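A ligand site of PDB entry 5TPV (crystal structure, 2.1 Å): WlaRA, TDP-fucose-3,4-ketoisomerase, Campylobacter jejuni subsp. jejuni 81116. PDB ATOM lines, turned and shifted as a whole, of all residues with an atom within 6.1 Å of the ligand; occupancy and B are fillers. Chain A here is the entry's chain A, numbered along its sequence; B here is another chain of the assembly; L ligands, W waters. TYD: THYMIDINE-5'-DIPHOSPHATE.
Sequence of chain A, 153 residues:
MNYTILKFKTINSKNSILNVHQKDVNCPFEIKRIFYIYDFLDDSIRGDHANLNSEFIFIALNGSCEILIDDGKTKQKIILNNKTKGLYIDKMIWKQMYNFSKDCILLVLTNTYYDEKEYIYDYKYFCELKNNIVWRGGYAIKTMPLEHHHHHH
NH2 of Arg 46 is in hydrogen-bond range of O of Ser 13 of chain B (3.2 Å). The backbone carbonyl oxygen (O) of Gly 47 sits at hydrogen-bond distance from the side-chain amino group (NZ) of Lys 14 of chain B, at 3.3 Å. The backbone NH (N) of Met 97 is in hydrogen-bond range of the backbone carbonyl oxygen (O) of Arg 46. The backbone NH (N) of Tyr 114 sits at hydrogen-bond distance from the side-chain amide oxygen (OE1) of Gln 22 of chain B (3.0 Å). The backbone carbonyl oxygen (O) of His 49 lies within hydrogen-bond range of the side-chain amino group (NZ) of Lys 95. The backbone NH (N) of Ile 11 of chain B lies within hydrogen-bond range of the backbone carbonyl oxygen (O) of Leu 18 of chain B, at 2.8 Å.
NH1 of Arg 46 is in salt-bridge range of O3B of the ligand, at 2.9 Å. The guanidinium group (NH2) of Arg 33 is in hydrogen-bond range of an oxygen (O4) of the ligand, 2.7 Å away. An oxygen (O2B) of the ligand is in salt-bridge range of the side-chain amino group (NZ) of Lys 14 of chain B. A ring nitrogen (NE2) of His 49 lies within hydrogen-bond range of an oxygen (O1B) of the ligand, 2.5 Å away. N of Gly 47 is in hydrogen-bond range of O2B of the ligand (2.8 Å). The side-chain hydroxyl (OH) of Tyr 119 lies within hydrogen-bond range of an oxygen (O1A) of the ligand (3.0 Å).
Phe 35 touches the ligand. Tyr 114 touches the ligand. CD1 of Ile 11 of chain B touches O2 of the ligand, 3.4 Å away. CD2 of Leu 18 of chain B touches O4' of the ligand, 3.5 Å away. Val 20 of chain B touches the ligand. Within 4 Å of the ligand: Arg 33, Phe 35, Arg 46, Gly 47, His 49, Tyr 114, Tyr 119, Ile 11 of chain B, Lys 14 of chain B, Leu 18 of chain B and Val 20 of chain B. The nearest printed residue that does not touch the ligand is Ile 37 (4.2 Å).
Water W3 bridges an oxygen (O1A) of the ligand (2.8 Å) and the side-chain hydroxyl (OH) of Tyr 119 (3.4 Å).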
ATOM      1  N   ARG A  33     -14.984  34.176  17.261  1.00  0.00           N
ATOM      2  CA  ARG A  33     -14.699  32.801  17.601  1.00  0.00           C
ATOM      3  C   ARG A  33     -15.895  31.919  17.203  1.00  0.00           C
ATOM      4  O   ARG A  33     -17.025  32.423  17.261  1.00  0.00           O
ATOM      5  CB  ARG A  33     -14.418  32.719  19.125  1.00  0.00           C
ATOM      6  CG  ARG A  33     -14.560  31.329  19.684  1.00  0.00           C
ATOM      7  CD  ARG A  33     -14.017  31.294  21.128  1.00  0.00           C
ATOM      8  NE  ARG A  33     -14.666  32.303  21.934  1.00  0.00           N
ATOM      9  CZ  ARG A  33     -15.319  32.076  23.079  1.00  0.00           C
ATOM     10  NH1 ARG A  33     -15.872  33.133  23.637  1.00  0.00           N
ATOM     11  NH2 ARG A  33     -15.418  30.853  23.619  1.00  0.00           N
ATOM     12  N   PHE A  35     -17.234  27.697  17.549  1.00  0.00           N
ATOM     13  CA  PHE A  35     -16.969  26.336  17.916  1.00  0.00           C
ATOM     14  C   PHE A  35     -18.163  25.453  17.623  1.00  0.00           C
ATOM     15  O   PHE A  35     -19.279  25.893  17.394  1.00  0.00           O
ATOM     16  CB  PHE A  35     -16.563  26.244  19.394  1.00  0.00           C
ATOM     17  CG  PHE A  35     -17.474  26.961  20.348  1.00  0.00           C
ATOM     18  CD1 PHE A  35     -18.494  26.268  20.988  1.00  0.00           C
ATOM     19  CD2 PHE A  35     -17.268  28.291  20.675  1.00  0.00           C
ATOM     20  CE1 PHE A  35     -19.279  26.899  21.946  1.00  0.00           C
ATOM     21  CE2 PHE A  35     -18.074  28.932  21.578  1.00  0.00           C
ATOM     22  CZ  PHE A  35     -19.062  28.215  22.251  1.00  0.00           C
ATOM     23  N   ILE A  37     -19.745  21.299  18.563  1.00  0.00           N
ATOM     24  CA  ILE A  37     -19.838  20.259  19.600  1.00  0.00           C
ATOM     25  C   ILE A  37     -20.575  19.090  18.976  1.00  0.00           C
ATOM     26  O   ILE A  37     -21.556  19.277  18.260  1.00  0.00           O
ATOM     27  CB  ILE A  37     -20.555  20.772  20.860  1.00  0.00           C
ATOM     28  CG1 ILE A  37     -20.042  22.173  21.209  1.00  0.00           C
ATOM     29  CG2 ILE A  37     -20.354  19.800  22.018  1.00  0.00           C
ATOM     30  CD1 ILE A  37     -20.547  22.815  22.456  1.00  0.00           C
ATOM     31  N   ILE A  45     -24.910  16.907  28.810  1.00  0.00           N
ATOM     32  CA  ILE A  45     -25.401  18.228  29.090  1.00  0.00           C
ATOM     33  C   ILE A  45     -24.225  19.191  28.919  1.00  0.00           C
ATOM     34  O   ILE A  45     -23.126  18.926  29.406  1.00  0.00           O
ATOM     35  CB  ILE A  45     -25.918  18.359  30.543  1.00  0.00           C
ATOM     36  CG1 ILE A  45     -26.904  17.233  30.879  1.00  0.00           C
ATOM     37  CG2 ILE A  45     -26.628  19.708  30.747  1.00  0.00           C
ATOM     38  CD1 ILE A  45     -27.404  17.295  32.313  1.00  0.00           C
ATOM     39  N   ARG A  46     -24.507  20.347  28.332  1.00  0.00           N
ATOM     40  CA  ARG A  46     -23.500  21.362  28.137  1.00  0.00           C
ATOM     41  C   ARG A  46     -24.079  22.617  28.718  1.00  0.00           C
ATOM     42  O   ARG A  46     -25.301  22.738  28.881  1.00  0.00           O
ATOM     43  CB  ARG A  46     -23.168  21.613  26.638  1.00  0.00           C
ATOM     44  CG  ARG A  46     -22.857  20.373  25.814  1.00  0.00           C
ATOM     45  CD  ARG A  46     -21.456  19.774  25.933  1.00  0.00           C
ATOM     46  NE  ARG A  46     -20.413  20.798  25.984  1.00  0.00           N
ATOM     47  CZ  ARG A  46     -19.131  20.545  25.763  1.00  0.00           C
ATOM     48  NH1 ARG A  46     -18.220  21.516  25.879  1.00  0.00           N
ATOM     49  NH2 ARG A  46     -18.760  19.348  25.373  1.00  0.00           N
ATOM     50  N   GLY A  47     -23.192  23.571  28.989  1.00  0.00           N
ATOM     51  CA  GLY A  47     -23.576  24.867  29.513  1.00  0.00           C
ATOM     52  C   GLY A  47     -23.507  24.832  31.037  1.00  0.00           C
ATOM     53  O   GLY A  47     -22.482  24.484  31.584  1.00  0.00           O
ATOM     54  N   ASP A  48     -24.584  25.231  31.714  1.00  0.00           N
ATOM     55  CA  ASP A  48     -24.544  25.539  33.158  1.00  0.00           C
ATOM     56  C   ASP A  48     -23.651  26.664  33.544  1.00  0.00           C
ATOM     57  O   ASP A  48     -22.990  26.570  34.561  1.00  0.00           O
ATOM     58  CB  ASP A  48     -24.128  24.355  34.014  1.00  0.00           C
ATOM     59  CG  ASP A  48     -25.222  23.339  34.097  1.00  0.00           C
ATOM     60  OD1 ASP A  48     -26.306  23.768  34.545  1.00  0.00           O
ATOM     61  OD2 ASP A  48     -24.998  22.188  33.679  1.00  0.00           O
ATOM     62  N   HIS A  49     -23.671  27.725  32.755  1.00  0.00           N
ATOM     63  CA  HIS A  49     -23.034  28.956  33.135  1.00  0.00           C
ATOM     64  C   HIS A  49     -23.663  30.108  32.386  1.00  0.00           C
ATOM     65  O   HIS A  49     -24.376  29.899  31.417  1.00  0.00           O
ATOM     66  CB  HIS A  49     -21.541  28.901  32.828  1.00  0.00           C
ATOM     67  CG  HIS A  49     -21.212  28.460  31.445  1.00  0.00           C
ATOM     68  ND1 HIS A  49     -21.221  29.343  30.369  1.00  0.00           N
ATOM     69  CD2 HIS A  49     -20.894  27.250  30.940  1.00  0.00           C
ATOM     70  CE1 HIS A  49     -20.851  28.687  29.288  1.00  0.00           C
ATOM     71  NE2 HIS A  49     -20.689  27.410  29.589  1.00  0.00           N
ATOM     72  N   LYS A  95     -27.684  29.241  30.554  1.00  0.00           N
ATOM     73  CA  LYS A  95     -28.163  28.330  29.550  1.00  0.00           C
ATOM     74  C   LYS A  95     -27.659  26.958  29.889  1.00  0.00           C
ATOM     75  O   LYS A  95     -26.585  26.802  30.468  1.00  0.00           O
ATOM     76  CB  LYS A  95     -27.792  28.761  28.124  1.00  0.00           C
ATOM     77  CG  LYS A  95     -26.485  28.181  27.599  1.00  0.00           C
ATOM     78  CD  LYS A  95     -25.208  28.734  28.210  1.00  0.00           C
ATOM     79  CE  LYS A  95     -25.149  30.253  28.108  1.00  0.00           C
ATOM     80  NZ  LYS A  95     -23.781  30.726  28.505  1.00  0.00           N
ATOM     81  N   MET A  97     -27.845  22.990  27.709  1.00  0.00           N
ATOM     82  CA  MET A  97     -28.130  22.339  26.476  1.00  0.00           C
ATOM     83  C   MET A  97     -28.099  20.861  26.760  1.00  0.00           C
ATOM     84  O   MET A  97     -27.224  20.412  27.476  1.00  0.00           O
ATOM     85  CB  MET A  97     -27.062  22.684  25.466  1.00  0.00           C
ATOM     86  CG  MET A  97     -27.262  24.089  24.976  1.00  0.00           C
ATOM     87  SD  MET A  97     -25.853  24.566  23.995  1.00  0.00           S
ATOM     88  CE  MET A  97     -24.755  24.891  25.410  1.00  0.00           C
ATOM     89  N   TYR A 114     -12.031  33.406  23.762  1.00  0.00           N
ATOM     90  CA  TYR A 114     -12.351  32.647  24.928  1.00  0.00           C
ATOM     91  C   TYR A 114     -11.660  33.261  26.198  1.00  0.00           C
ATOM     92  O   TYR A 114     -10.488  33.598  26.174  1.00  0.00           O
ATOM     93  CB  TYR A 114     -11.893  31.221  24.736  1.00  0.00           C
ATOM     94  CG  TYR A 114     -11.858  30.459  26.037  1.00  0.00           C
ATOM     95  CD1 TYR A 114     -10.674  30.264  26.721  1.00  0.00           C
ATOM     96  CD2 TYR A 114     -13.033  29.957  26.595  1.00  0.00           C
ATOM     97  CE1 TYR A 114     -10.647  29.581  27.919  1.00  0.00           C
ATOM     98  CE2 TYR A 114     -13.020  29.258  27.787  1.00  0.00           C
ATOM     99  CZ  TYR A 114     -11.822  29.106  28.441  1.00  0.00           C
ATOM    100  OH  TYR A 114     -11.804  28.428  29.603  1.00  0.00           O
ATOM    101  N   TYR A 119     -16.822  33.938  32.928  1.00  0.00           N
ATOM    102  CA  TYR A 119     -17.824  32.974  33.279  1.00  0.00           C
ATOM    103  C   TYR A 119     -18.361  33.137  34.682  1.00  0.00           C
ATOM    104  O   TYR A 119     -17.612  33.441  35.628  1.00  0.00           O
ATOM    105  CB  TYR A 119     -17.225  31.580  33.257  1.00  0.00           C
ATOM    106  CG  TYR A 119     -17.064  30.908  31.913  1.00  0.00           C
ATOM    107  CD1 TYR A 119     -16.272  31.466  30.936  1.00  0.00           C
ATOM    108  CD2 TYR A 119     -17.646  29.675  31.649  1.00  0.00           C
ATOM    109  CE1 TYR A 119     -16.077  30.833  29.715  1.00  0.00           C
ATOM    110  CE2 TYR A 119     -17.488  29.045  30.425  1.00  0.00           C
ATOM    111  CZ  TYR A 119     -16.689  29.640  29.464  1.00  0.00           C
ATOM    112  OH  TYR A 119     -16.485  29.029  28.244  1.00  0.00           O
ATOM    113  N   TYR A 121     -20.271  30.634  37.119  1.00  0.00           N
ATOM    114  CA  TYR A 121     -20.752  29.276  37.376  1.00  0.00           C
ATOM    115  C   TYR A 121     -21.664  29.085  38.558  1.00  0.00           C
ATOM    116  O   TYR A 121     -22.181  27.970  38.766  1.00  0.00           O
ATOM    117  CB  TYR A 121     -19.600  28.344  37.657  1.00  0.00           C
ATOM    118  CG  TYR A 121     -18.593  28.257  36.560  1.00  0.00           C
ATOM    119  CD1 TYR A 121     -18.790  27.402  35.471  1.00  0.00           C
ATOM    120  CD2 TYR A 121     -17.440  29.002  36.622  1.00  0.00           C
ATOM    121  CE1 TYR A 121     -17.842  27.305  34.450  1.00  0.00           C
ATOM    122  CE2 TYR A 121     -16.491  28.914  35.623  1.00  0.00           C
ATOM    123  CZ  TYR A 121     -16.687  28.067  34.558  1.00  0.00           C
ATOM    124  OH  TYR A 121     -15.695  28.057  33.607  1.00  0.00           O
ATOM    125  N   ILE B  11     -11.388  19.343  22.548  1.00  0.00           N
ATOM    126  CA  ILE B  11     -11.681  19.271  23.979  1.00  0.00           C
ATOM    127  C   ILE B  11     -12.761  18.226  24.285  1.00  0.00           C
ATOM    128  O   ILE B  11     -13.976  18.411  24.027  1.00  0.00           O
ATOM    129  CB  ILE B  11     -12.056  20.634  24.548  1.00  0.00           C
ATOM    130  CG1 ILE B  11     -10.944  21.656  24.275  1.00  0.00           C
ATOM    131  CG2 ILE B  11     -12.221  20.559  26.061  1.00  0.00           C
ATOM    132  CD1 ILE B  11     -11.356  23.094  24.448  1.00  0.00           C
ATOM    133  N   SER B  13     -14.979  16.293  26.708  1.00  0.00           N
ATOM    134  CA  SER B  13     -15.535  16.522  28.048  1.00  0.00           C
ATOM    135  C   SER B  13     -17.062  16.584  28.014  1.00  0.00           C
ATOM    136  O   SER B  13     -17.678  16.774  26.969  1.00  0.00           O
ATOM    137  CB  SER B  13     -14.956  17.755  28.729  1.00  0.00           C
ATOM    138  OG  SER B  13     -15.518  18.988  28.309  1.00  0.00           O
ATOM    139  N   LYS B  14     -17.671  16.369  29.158  1.00  0.00           N
ATOM    140  CA  LYS B  14     -19.104  16.283  29.227  1.00  0.00           C
ATOM    141  C   LYS B  14     -19.722  15.361  28.180  1.00  0.00           C
ATOM    142  O   LYS B  14     -20.692  15.731  27.510  1.00  0.00           O
ATOM    143  CB  LYS B  14     -19.690  17.694  29.133  1.00  0.00           C
ATOM    144  CG  LYS B  14     -18.969  18.745  29.976  1.00  0.00           C
ATOM    145  CD  LYS B  14     -19.719  20.068  29.905  1.00  0.00           C
ATOM    146  CE  LYS B  14     -19.332  21.058  30.983  1.00  0.00           C
ATOM    147  NZ  LYS B  14     -20.130  22.322  30.840  1.00  0.00           N
ATOM    148  N   LEU B  18     -15.739  19.054  21.693  1.00  0.00           N
ATOM    149  CA  LEU B  18     -15.801  20.461  21.345  1.00  0.00           C
ATOM    150  C   LEU B  18     -14.566  20.813  20.525  1.00  0.00           C
ATOM    151  O   LEU B  18     -13.474  20.422  20.941  1.00  0.00           O
ATOM    152  CB  LEU B  18     -15.755  21.265  22.606  1.00  0.00           C
ATOM    153  CG  LEU B  18     -15.463  22.754  22.522  1.00  0.00           C
ATOM    154  CD1 LEU B  18     -16.612  23.481  21.854  1.00  0.00           C
ATOM    155  CD2 LEU B  18     -15.296  23.310  23.939  1.00  0.00           C
ATOM    156  N   VAL B  20     -12.727  24.203  18.998  1.00  0.00           N
ATOM    157  CA  VAL B  20     -12.757  25.662  19.034  1.00  0.00           C
ATOM    158  C   VAL B  20     -11.902  26.277  17.933  1.00  0.00           C
ATOM    159  O   VAL B  20     -10.799  25.795  17.651  1.00  0.00           O
ATOM    160  CB  VAL B  20     -12.292  26.199  20.423  1.00  0.00           C
ATOM    161  CG1 VAL B  20     -12.393  27.703  20.503  1.00  0.00           C
ATOM    162  CG2 VAL B  20     -13.170  25.647  21.554  1.00  0.00           C
ATOM    163  N   GLN B  22     -10.468  30.140  16.775  1.00  0.00           N
ATOM    164  CA  GLN B  22     -10.268  31.584  16.847  1.00  0.00           C
ATOM    165  C   GLN B  22      -8.782  31.869  16.537  1.00  0.00           C
ATOM    166  O   GLN B  22      -7.987  30.942  16.440  1.00  0.00           O
ATOM    167  CB  GLN B  22     -10.591  32.111  18.233  1.00  0.00           C
ATOM    168  CG  GLN B  22      -9.694  31.541  19.311  1.00  0.00           C
ATOM    169  CD  GLN B  22      -9.944  32.175  20.677  1.00  0.00           C
ATOM    170  OE1 GLN B  22     -11.099  32.346  21.105  1.00  0.00           O
ATOM    171  NE2 GLN B  22      -8.880  32.531  21.373  1.00  0.00           N
HETATM  172  PA  TYD L   1     -17.548  25.346  28.763  1.00  0.00           P
HETATM  173  O1A TYD L   1     -18.113  26.550  28.054  1.00  0.00           O
HETATM  174  O2A TYD L   1     -17.170  25.436  30.220  1.00  0.00           O
HETATM  175  O3A TYD L   1     -18.578  24.124  28.588  1.00  0.00           O
HETATM  176  PB  TYD L   1     -19.840  24.252  27.596  1.00  0.00           P
HETATM  177  O1B TYD L   1     -20.477  25.569  27.984  1.00  0.00           O
HETATM  178  O2B TYD L   1     -20.690  23.040  27.915  1.00  0.00           O
HETATM  179  O3B TYD L   1     -19.232  24.241  26.218  1.00  0.00           O
HETATM  180  O5' TYD L   1     -16.261  24.834  27.932  1.00  0.00           O
HETATM  181  C5' TYD L   1     -15.885  23.461  27.968  1.00  0.00           C
HETATM  182  C4' TYD L   1     -14.389  23.349  28.221  1.00  0.00           C
HETATM  183  O4' TYD L   1     -13.671  23.602  27.011  1.00  0.00           O
HETATM  184  C3' TYD L   1     -13.925  24.360  29.254  1.00  0.00           C
HETATM  185  O3' TYD L   1     -13.342  23.686  30.374  1.00  0.00           O
HETATM  186  C2' TYD L   1     -12.884  25.232  28.574  1.00  0.00           C
HETATM  187  C1' TYD L   1     -12.766  24.708  27.156  1.00  0.00           C
HETATM  188  N1  TYD L   1     -13.111  25.760  26.201  1.00  0.00           N
HETATM  189  C2  TYD L   1     -12.083  26.490  25.560  1.00  0.00           C
HETATM  190  O2  TYD L   1     -10.895  26.223  25.818  1.00  0.00           O
HETATM  191  N3  TYD L   1     -12.364  27.460  24.685  1.00  0.00           N
HETATM  192  C4  TYD L   1     -13.627  27.773  24.383  1.00  0.00           C
HETATM  193  O4  TYD L   1     -13.882  28.678  23.566  1.00  0.00           O
HETATM  194  C5  TYD L   1     -14.722  27.023  25.047  1.00  0.00           C
HETATM  195  C5M TYD L   1     -16.166  27.343  24.732  1.00  0.00           C
HETATM  196  C6  TYD L   1     -14.402  26.022  25.945  1.00  0.00           C
HETATM  197  O   HOH W   1     -22.100  26.600  25.427  1.00  0.00           O
HETATM  198  O   HOH W   2      -9.971  28.535  23.209  1.00  0.00           O
HETATM  199  O   HOH W   3     -19.330  28.516  26.417  1.00  0.00           O
